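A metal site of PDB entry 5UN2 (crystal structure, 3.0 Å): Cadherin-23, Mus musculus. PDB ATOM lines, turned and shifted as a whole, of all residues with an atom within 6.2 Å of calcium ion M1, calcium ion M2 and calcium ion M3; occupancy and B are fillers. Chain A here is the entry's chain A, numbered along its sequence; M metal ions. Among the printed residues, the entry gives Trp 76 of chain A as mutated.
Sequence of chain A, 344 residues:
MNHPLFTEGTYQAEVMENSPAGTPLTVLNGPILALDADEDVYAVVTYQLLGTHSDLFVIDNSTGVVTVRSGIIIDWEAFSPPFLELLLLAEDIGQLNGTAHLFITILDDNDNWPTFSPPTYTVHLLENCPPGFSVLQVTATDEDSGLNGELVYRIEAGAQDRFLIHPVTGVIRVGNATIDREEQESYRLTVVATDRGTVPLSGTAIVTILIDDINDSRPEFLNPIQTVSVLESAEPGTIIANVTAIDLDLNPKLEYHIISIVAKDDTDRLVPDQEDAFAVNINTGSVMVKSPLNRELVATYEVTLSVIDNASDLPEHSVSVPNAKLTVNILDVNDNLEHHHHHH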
ATOM      1  N   GLU A  17     -33.790  -5.218 -25.876  1.00  0.00           N
ATOM      2  CA  GLU A  17     -33.546  -3.775 -25.816  1.00  0.00           C
ATOM      3  C   GLU A  17     -32.312  -3.414 -26.679  1.00  0.00           C
ATOM      4  O   GLU A  17     -31.437  -4.267 -26.868  1.00  0.00           O
ATOM      5  CB  GLU A  17     -33.390  -3.285 -24.350  1.00  0.00           C
ATOM      6  CG  GLU A  17     -32.149  -3.807 -23.589  1.00  0.00           C
ATOM      7  CD  GLU A  17     -31.780  -2.997 -22.333  1.00  0.00           C
ATOM      8  OE1 GLU A  17     -31.312  -3.615 -21.345  1.00  0.00           O
ATOM      9  OE2 GLU A  17     -31.932  -1.745 -22.325  1.00  0.00           O
ATOM     10  N   ASN A  18     -32.268  -2.176 -27.192  1.00  0.00           N
ATOM     11  CA  ASN A  18     -31.176  -1.693 -28.100  1.00  0.00           C
ATOM     12  C   ASN A  18     -31.082  -2.400 -29.482  1.00  0.00           C
ATOM     13  O   ASN A  18     -30.043  -2.320 -30.137  1.00  0.00           O
ATOM     14  CB  ASN A  18     -29.792  -1.729 -27.415  1.00  0.00           C
ATOM     15  CG  ASN A  18     -29.846  -1.315 -25.948  1.00  0.00           C
ATOM     16  OD1 ASN A  18     -30.436  -0.287 -25.602  1.00  0.00           O
ATOM     17  ND2 ASN A  18     -29.232  -2.128 -25.084  1.00  0.00           N
ATOM     18  N   ILE A  74     -35.203   1.214 -27.754  1.00  0.00           N
ATOM     19  CA  ILE A  74     -35.880   0.351 -26.767  1.00  0.00           C
ATOM     20  C   ILE A  74     -34.986   0.287 -25.511  1.00  0.00           C
ATOM     21  O   ILE A  74     -33.857  -0.212 -25.583  1.00  0.00           O
ATOM     22  CB  ILE A  74     -36.070  -1.106 -27.287  1.00  0.00           C
ATOM     23  CG1 ILE A  74     -36.738  -1.175 -28.670  1.00  0.00           C
ATOM     24  CG2 ILE A  74     -36.842  -1.943 -26.288  1.00  0.00           C
ATOM     25  CD1 ILE A  74     -38.134  -0.594 -28.746  1.00  0.00           C
ATOM     26  N   ASP A  75     -35.481   0.787 -24.372  1.00  0.00           N
ATOM     27  CA  ASP A  75     -34.721   0.846 -23.102  1.00  0.00           C
ATOM     28  C   ASP A  75     -35.415   0.013 -22.002  1.00  0.00           C
ATOM     29  O   ASP A  75     -36.462   0.419 -21.483  1.00  0.00           O
ATOM     30  CB  ASP A  75     -34.599   2.321 -22.684  1.00  0.00           C
ATOM     31  CG  ASP A  75     -33.556   2.552 -21.609  1.00  0.00           C
ATOM     32  OD1 ASP A  75     -33.295   1.657 -20.786  1.00  0.00           O
ATOM     33  OD2 ASP A  75     -33.000   3.656 -21.590  1.00  0.00           O
ATOM     34  N   TRP A  76     -34.821  -1.136 -21.638  1.00  0.00           N
ATOM     35  CA  TRP A  76     -35.364  -2.002 -20.558  1.00  0.00           C
ATOM     36  C   TRP A  76     -35.490  -1.252 -19.244  1.00  0.00           C
ATOM     37  O   TRP A  76     -36.481  -1.428 -18.521  1.00  0.00           O
ATOM     38  CB  TRP A  76     -34.474  -3.229 -20.331  1.00  0.00           C
ATOM     39  CG  TRP A  76     -35.098  -4.273 -19.435  1.00  0.00           C
ATOM     40  CD1 TRP A  76     -35.812  -5.335 -19.829  1.00  0.00           C
ATOM     41  CD2 TRP A  76     -35.037  -4.338 -18.008  1.00  0.00           C
ATOM     42  NE1 TRP A  76     -36.211  -6.076 -18.752  1.00  0.00           N
ATOM     43  CE2 TRP A  76     -35.753  -5.481 -17.611  1.00  0.00           C
ATOM     44  CE3 TRP A  76     -34.452  -3.544 -17.013  1.00  0.00           C
ATOM     45  CZ2 TRP A  76     -35.915  -5.853 -16.285  1.00  0.00           C
ATOM     46  CZ3 TRP A  76     -34.606  -3.909 -15.688  1.00  0.00           C
ATOM     47  CH2 TRP A  76     -35.342  -5.053 -15.339  1.00  0.00           C
ATOM     48  N   GLU A  77     -34.494  -0.421 -18.951  1.00  0.00           N
ATOM     49  CA  GLU A  77     -34.432   0.340 -17.693  1.00  0.00           C
ATOM     50  C   GLU A  77     -35.473   1.465 -17.603  1.00  0.00           C
ATOM     51  O   GLU A  77     -35.690   1.994 -16.502  1.00  0.00           O
ATOM     52  CB  GLU A  77     -33.024   0.913 -17.466  1.00  0.00           C
ATOM     53  CG  GLU A  77     -31.966  -0.095 -17.037  1.00  0.00           C
ATOM     54  CD  GLU A  77     -31.443  -0.941 -18.188  1.00  0.00           C
ATOM     55  OE1 GLU A  77     -31.042  -0.377 -19.240  1.00  0.00           O
ATOM     56  OE2 GLU A  77     -31.404  -2.178 -18.030  1.00  0.00           O
ATOM     57  N   ALA A  78     -36.106   1.825 -18.732  1.00  0.00           N
ATOM     58  CA  ALA A  78     -37.133   2.870 -18.792  1.00  0.00           C
ATOM     59  C   ALA A  78     -38.610   2.394 -18.650  1.00  0.00           C
ATOM     60  O   ALA A  78     -39.511   3.220 -18.518  1.00  0.00           O
ATOM     61  CB  ALA A  78     -36.961   3.677 -20.074  1.00  0.00           C
ATOM     62  N   ASP A 108     -33.895  -7.860 -21.199  1.00  0.00           N
ATOM     63  CA  ASP A 108     -32.792  -7.091 -20.625  1.00  0.00           C
ATOM     64  C   ASP A 108     -31.482  -7.457 -21.312  1.00  0.00           C
ATOM     65  O   ASP A 108     -31.263  -8.611 -21.625  1.00  0.00           O
ATOM     66  CB  ASP A 108     -32.684  -7.378 -19.116  1.00  0.00           C
ATOM     67  CG  ASP A 108     -31.560  -6.600 -18.444  1.00  0.00           C
ATOM     68  OD1 ASP A 108     -31.298  -5.453 -18.851  1.00  0.00           O
ATOM     69  OD2 ASP A 108     -30.937  -7.146 -17.489  1.00  0.00           O
ATOM     70  N   ASP A 109     -30.635  -6.450 -21.560  1.00  0.00           N
ATOM     71  CA  ASP A 109     -29.251  -6.685 -22.019  1.00  0.00           C
ATOM     72  C   ASP A 109     -28.275  -6.004 -21.062  1.00  0.00           C
ATOM     73  O   ASP A 109     -28.588  -4.955 -20.491  1.00  0.00           O
ATOM     74  CB  ASP A 109     -29.033  -6.162 -23.449  1.00  0.00           C
ATOM     75  CG  ASP A 109     -27.649  -6.530 -24.004  1.00  0.00           C
ATOM     76  OD1 ASP A 109     -27.151  -7.645 -23.750  1.00  0.00           O
ATOM     77  OD2 ASP A 109     -27.052  -5.687 -24.698  1.00  0.00           O
ATOM     78  N   ASN A 110     -27.099  -6.611 -20.885  1.00  0.00           N
ATOM     79  CA  ASN A 110     -26.085  -6.100 -19.977  1.00  0.00           C
ATOM     80  C   ASN A 110     -25.493  -4.823 -20.564  1.00  0.00           C
ATOM     81  O   ASN A 110     -24.472  -4.856 -21.254  1.00  0.00           O
ATOM     82  CB  ASN A 110     -25.009  -7.170 -19.741  1.00  0.00           C
ATOM     83  CG  ASN A 110     -24.059  -6.826 -18.607  1.00  0.00           C
ATOM     84  OD1 ASN A 110     -24.348  -5.980 -17.759  1.00  0.00           O
ATOM     85  ND2 ASN A 110     -22.917  -7.487 -18.585  1.00  0.00           N
ATOM     86  N   ASP A 111     -26.161  -3.699 -20.311  1.00  0.00           N
ATOM     87  CA  ASP A 111     -25.783  -2.411 -20.900  1.00  0.00           C
ATOM     88  C   ASP A 111     -25.676  -1.268 -19.883  1.00  0.00           C
ATOM     89  O   ASP A 111     -25.814  -0.094 -20.248  1.00  0.00           O
ATOM     90  CB  ASP A 111     -26.759  -2.039 -22.034  1.00  0.00           C
ATOM     91  CG  ASP A 111     -28.190  -1.754 -21.541  1.00  0.00           C
ATOM     92  OD1 ASP A 111     -28.543  -2.032 -20.384  1.00  0.00           O
ATOM     93  OD2 ASP A 111     -28.979  -1.245 -22.352  1.00  0.00           O
ATOM     94  N   ASN A 112     -25.424  -1.605 -18.613  1.00  0.00           N
ATOM     95  CA  ASN A 112     -25.097  -0.609 -17.590  1.00  0.00           C
ATOM     96  C   ASN A 112     -23.830  -1.043 -16.866  1.00  0.00           C
ATOM     97  O   ASN A 112     -23.683  -2.211 -16.503  1.00  0.00           O
ATOM     98  CB  ASN A 112     -26.244  -0.403 -16.597  1.00  0.00           C
ATOM     99  CG  ASN A 112     -27.402   0.373 -17.186  1.00  0.00           C
ATOM    100  OD1 ASN A 112     -27.633   1.525 -16.801  1.00  0.00           O
ATOM    101  ND2 ASN A 112     -28.135  -0.235 -18.107  1.00  0.00           N
ATOM    102  N   TRP A 113     -22.937  -0.082 -16.664  1.00  0.00           N
ATOM    103  CA  TRP A 113     -21.617  -0.324 -16.105  1.00  0.00           C
ATOM    104  C   TRP A 113     -21.737  -0.206 -14.589  1.00  0.00           C
ATOM    105  O   TRP A 113     -22.363   0.747 -14.114  1.00  0.00           O
ATOM    106  CB  TRP A 113     -20.612   0.700 -16.647  1.00  0.00           C
ATOM    107  CG  TRP A 113     -20.401   0.587 -18.135  1.00  0.00           C
ATOM    108  CD1 TRP A 113     -21.286   0.919 -19.139  1.00  0.00           C
ATOM    109  CD2 TRP A 113     -19.225   0.102 -18.800  1.00  0.00           C
ATOM    110  NE1 TRP A 113     -20.730   0.664 -20.375  1.00  0.00           N
ATOM    111  CE2 TRP A 113     -19.469   0.161 -20.193  1.00  0.00           C
ATOM    112  CE3 TRP A 113     -17.983  -0.384 -18.343  1.00  0.00           C
ATOM    113  CZ2 TRP A 113     -18.506  -0.241 -21.145  1.00  0.00           C
ATOM    114  CZ3 TRP A 113     -17.027  -0.793 -19.284  1.00  0.00           C
ATOM    115  CH2 TRP A 113     -17.290  -0.710 -20.675  1.00  0.00           C
ATOM    116  N   PRO A 114     -21.175  -1.167 -13.814  1.00  0.00           N
ATOM    117  CA  PRO A 114     -21.184  -1.022 -12.354  1.00  0.00           C
ATOM    118  C   PRO A 114     -20.559   0.287 -11.936  1.00  0.00           C
ATOM    119  O   PRO A 114     -19.386   0.493 -12.180  1.00  0.00           O
ATOM    120  CB  PRO A 114     -20.323  -2.212 -11.883  1.00  0.00           C
ATOM    121  CG  PRO A 114     -20.456  -3.219 -12.951  1.00  0.00           C
ATOM    122  CD  PRO A 114     -20.559  -2.436 -14.226  1.00  0.00           C
ATOM    123  N   ASP A 142     -25.868  -0.793 -10.073  1.00  0.00           N
ATOM    124  CA  ASP A 142     -26.051  -1.324 -11.423  1.00  0.00           C
ATOM    125  C   ASP A 142     -27.564  -1.362 -11.756  1.00  0.00           C
ATOM    126  O   ASP A 142     -28.348  -2.071 -11.082  1.00  0.00           O
ATOM    127  CB  ASP A 142     -25.417  -2.715 -11.521  1.00  0.00           C
ATOM    128  CG  ASP A 142     -25.121  -3.148 -12.938  1.00  0.00           C
ATOM    129  OD1 ASP A 142     -25.863  -2.772 -13.872  1.00  0.00           O
ATOM    130  OD2 ASP A 142     -24.140  -3.893 -13.134  1.00  0.00           O
ATOM    131  N   GLU A 143     -27.943  -0.621 -12.790  1.00  0.00           N
ATOM    132  CA  GLU A 143     -29.350  -0.533 -13.202  1.00  0.00           C
ATOM    133  C   GLU A 143     -29.820  -1.703 -14.058  1.00  0.00           C
ATOM    134  O   GLU A 143     -30.988  -1.749 -14.436  1.00  0.00           O
ATOM    135  CB  GLU A 143     -29.638   0.791 -13.925  1.00  0.00           C
ATOM    136  CG  GLU A 143     -29.205   2.040 -13.157  1.00  0.00           C
ATOM    137  CD  GLU A 143     -29.671   2.045 -11.712  1.00  0.00           C
ATOM    138  OE1 GLU A 143     -30.891   2.144 -11.463  1.00  0.00           O
ATOM    139  OE2 GLU A 143     -28.801   1.938 -10.815  1.00  0.00           O
ATOM    140  N   ASP A 144     -28.927  -2.650 -14.357  1.00  0.00           N
ATOM    141  CA  ASP A 144     -29.317  -3.898 -15.009  1.00  0.00           C
ATOM    142  C   ASP A 144     -30.055  -4.833 -14.041  1.00  0.00           C
ATOM    143  O   ASP A 144     -30.139  -4.550 -12.849  1.00  0.00           O
ATOM    144  CB  ASP A 144     -28.078  -4.607 -15.584  1.00  0.00           C
ATOM    145  CG  ASP A 144     -27.517  -3.921 -16.792  1.00  0.00           C
ATOM    146  OD1 ASP A 144     -28.317  -3.506 -17.659  1.00  0.00           O
ATOM    147  OD2 ASP A 144     -26.277  -3.823 -16.910  1.00  0.00           O
ATOM    148  N   SER A 145     -30.572  -5.933 -14.601  1.00  0.00           N
ATOM    149  CA  SER A 145     -31.348  -6.932 -13.858  1.00  0.00           C
ATOM    150  C   SER A 145     -30.677  -8.291 -13.810  1.00  0.00           C
ATOM    151  O   SER A 145     -29.885  -8.628 -14.702  1.00  0.00           O
ATOM    152  CB  SER A 145     -32.723  -7.108 -14.497  1.00  0.00           C
ATOM    153  OG  SER A 145     -32.653  -7.951 -15.649  1.00  0.00           O
ATOM    154  N   LEU A 147     -28.429 -11.379 -13.247  1.00  0.00           N
ATOM    155  CA  LEU A 147     -26.978 -11.510 -13.173  1.00  0.00           C
ATOM    156  C   LEU A 147     -26.252 -10.297 -13.725  1.00  0.00           C
ATOM    157  O   LEU A 147     -25.130 -10.023 -13.309  1.00  0.00           O
ATOM    158  CB  LEU A 147     -26.499 -12.777 -13.870  1.00  0.00           C
ATOM    159  CG  LEU A 147     -26.791 -14.096 -13.140  1.00  0.00           C
ATOM    160  CD1 LEU A 147     -26.313 -15.250 -14.003  1.00  0.00           C
ATOM    161  CD2 LEU A 147     -26.150 -14.138 -11.751  1.00  0.00           C
ATOM    162  N   ASN A 148     -26.887  -9.561 -14.625  1.00  0.00           N
ATOM    163  CA  ASN A 148     -26.269  -8.365 -15.212  1.00  0.00           C
ATOM    164  C   ASN A 148     -26.139  -7.191 -14.220  1.00  0.00           C
ATOM    165  O   ASN A 148     -25.416  -6.227 -14.490  1.00  0.00           O
ATOM    166  CB  ASN A 148     -27.050  -7.922 -16.456  1.00  0.00           C
ATOM    167  CG  ASN A 148     -27.314  -9.051 -17.422  1.00  0.00           C
ATOM    168  OD1 ASN A 148     -26.476  -9.945 -17.644  1.00  0.00           O
ATOM    169  ND2 ASN A 148     -28.502  -9.034 -18.021  1.00  0.00           N
ATOM    170  N   GLY A 149     -26.874  -7.256 -13.110  1.00  0.00           N
ATOM    171  CA  GLY A 149     -26.750  -6.324 -11.988  1.00  0.00           C
ATOM    172  C   GLY A 149     -25.997  -6.837 -10.778  1.00  0.00           C
ATOM    173  O   GLY A 149     -25.474  -6.040  -9.997  1.00  0.00           O
ATOM    174  N   LEU A 151     -23.152  -7.855  -8.629  1.00  0.00           N
ATOM    175  CA  LEU A 151     -21.771  -7.349  -8.648  1.00  0.00           C
ATOM    176  C   LEU A 151     -20.797  -8.148  -7.792  1.00  0.00           C
ATOM    177  O   LEU A 151     -21.154  -8.652  -6.738  1.00  0.00           O
ATOM    178  CB  LEU A 151     -21.730  -5.890  -8.178  1.00  0.00           C
ATOM    179  CG  LEU A 151     -22.459  -4.803  -8.967  1.00  0.00           C
ATOM    180  CD1 LEU A 151     -22.115  -3.446  -8.382  1.00  0.00           C
ATOM    181  CD2 LEU A 151     -22.101  -4.840 -10.446  1.00  0.00           C
ATOM    182  N   ASP A 195     -19.766  -6.936 -13.108  1.00  0.00           N
ATOM    183  CA  ASP A 195     -21.056  -7.644 -13.185  1.00  0.00           C
ATOM    184  C   ASP A 195     -20.869  -9.088 -13.695  1.00  0.00           C
ATOM    185  O   ASP A 195     -19.803  -9.426 -14.240  1.00  0.00           O
ATOM    186  CB  ASP A 195     -22.097  -6.863 -13.991  1.00  0.00           C
ATOM    187  CG  ASP A 195     -21.766  -6.769 -15.472  1.00  0.00           C
ATOM    188  OD1 ASP A 195     -21.746  -7.797 -16.166  1.00  0.00           O
ATOM    189  OD2 ASP A 195     -21.582  -5.639 -15.969  1.00  0.00           O
ATOM    190  N   LEU A 201     -19.345  -6.270 -17.789  1.00  0.00           N
ATOM    191  CA  LEU A 201     -18.765  -4.940 -17.629  1.00  0.00           C
ATOM    192  C   LEU A 201     -18.247  -4.738 -16.201  1.00  0.00           C
ATOM    193  O   LEU A 201     -18.634  -5.459 -15.277  1.00  0.00           O
ATOM    194  CB  LEU A 201     -19.794  -3.862 -18.014  1.00  0.00           C
ATOM    195  CG  LEU A 201     -20.476  -4.057 -19.380  1.00  0.00           C
ATOM    196  CD1 LEU A 201     -21.628  -3.089 -19.552  1.00  0.00           C
ATOM    197  CD2 LEU A 201     -19.470  -3.918 -20.518  1.00  0.00           C
HETATM  198 CA    CA M   1     -30.882   0.242 -21.604  1.00  0.00          CA
HETATM  199 CA    CA M   2     -30.066  -3.511 -19.303  1.00  0.00          CA
HETATM  200 CA    CA M   3     -24.165  -4.524 -15.845  1.00  0.00          CA
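The side-chain amide nitrogen (ND2) of Asn 112 sits close to the side-chain carboxylate (OE1) of Glu 77 (3.1 Å). N of Glu 77 sits at hydrogen-bond distance from OD1 of Asp 75 (3.0 Å). The side-chain carboxylate (OD2) of Asp 108 sits at hydrogen-bond distance from the side-chain amide nitrogen (ND2) of Asn 148 (3.1 Å). The side-chain hydroxyl (OG) of Ser 145 sits at hydrogen-bond distance from the side-chain carboxylate (OD2) of Asp 108, 2.6 Å away. The side-chain carboxylate (OE2) of Glu 17 lies close to the backbone NH (N) of Trp 76. The side-chain carboxylate of Asp 111 sits close to the side-chain amide nitrogen of Asn 18. The backbone NH (N) of Asp 195 is in hydrogen-bond range of the backbone carbonyl oxygen (O) of Leu 201 (2.9 Å). The side-chain carboxylate (OD1) of Asp 75 is in hydrogen-bond range of the backbone NH (N) of Ala 78 (3.5 Å).
Seven residues have an atom within 4 Å of calcium ion M2: Glu 17, Glu 77, Asp 108, Asp 109, Asp 111, Asn 112 and Asp 144.
Within 4 Å of calcium ion M3: Asn 110, Asn 112, Asp 142, Asp 144, Asn 148 and Asp 195.
Calcium ion M1 is bound by the side-chain carboxylate (OE2) of Glu 17 (2.4 Å), the side-chain carboxylate (OE1) of Glu 77 (2.4 Å) and the side-chain carboxylate (OD2) of Asp 111 (2.5 Å). Calcium ion M1 has three donor atoms within binding distance. Slightly farther from calcium ion M1 lies the side-chain carboxylate (OD1) of Asp 75 (2.9 Å).
Calcium ion M2 is bound by OE2 of Glu 77 (2.3 Å), OD1 of Asp 108 (2.3 Å), OD1 of Asp 111 (2.4 Å), O of Asp 109 (2.4 Å), OE1 of Glu 17 (2.4 Å) and OD1 of Asp 144 (2.4 Å). Calcium ion M2 has six donor atoms within binding distance.
Calcium ion M3 is bound by OD1 of Asn 110 (2.4 Å), O of Asn 112 (2.5 Å), OD2 of Asp 144 (2.5 Å), O of Asn 148 (2.5 Å), OD2 of Asp 142 (2.8 Å) and OD2 of Asp 195 (2.8 Å). Calcium ion M3 has six donor atoms within binding distance. Slightly farther from calcium ion M3 lies the side-chain carboxylate (OD1) of Asp 142 (3.1 Å).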
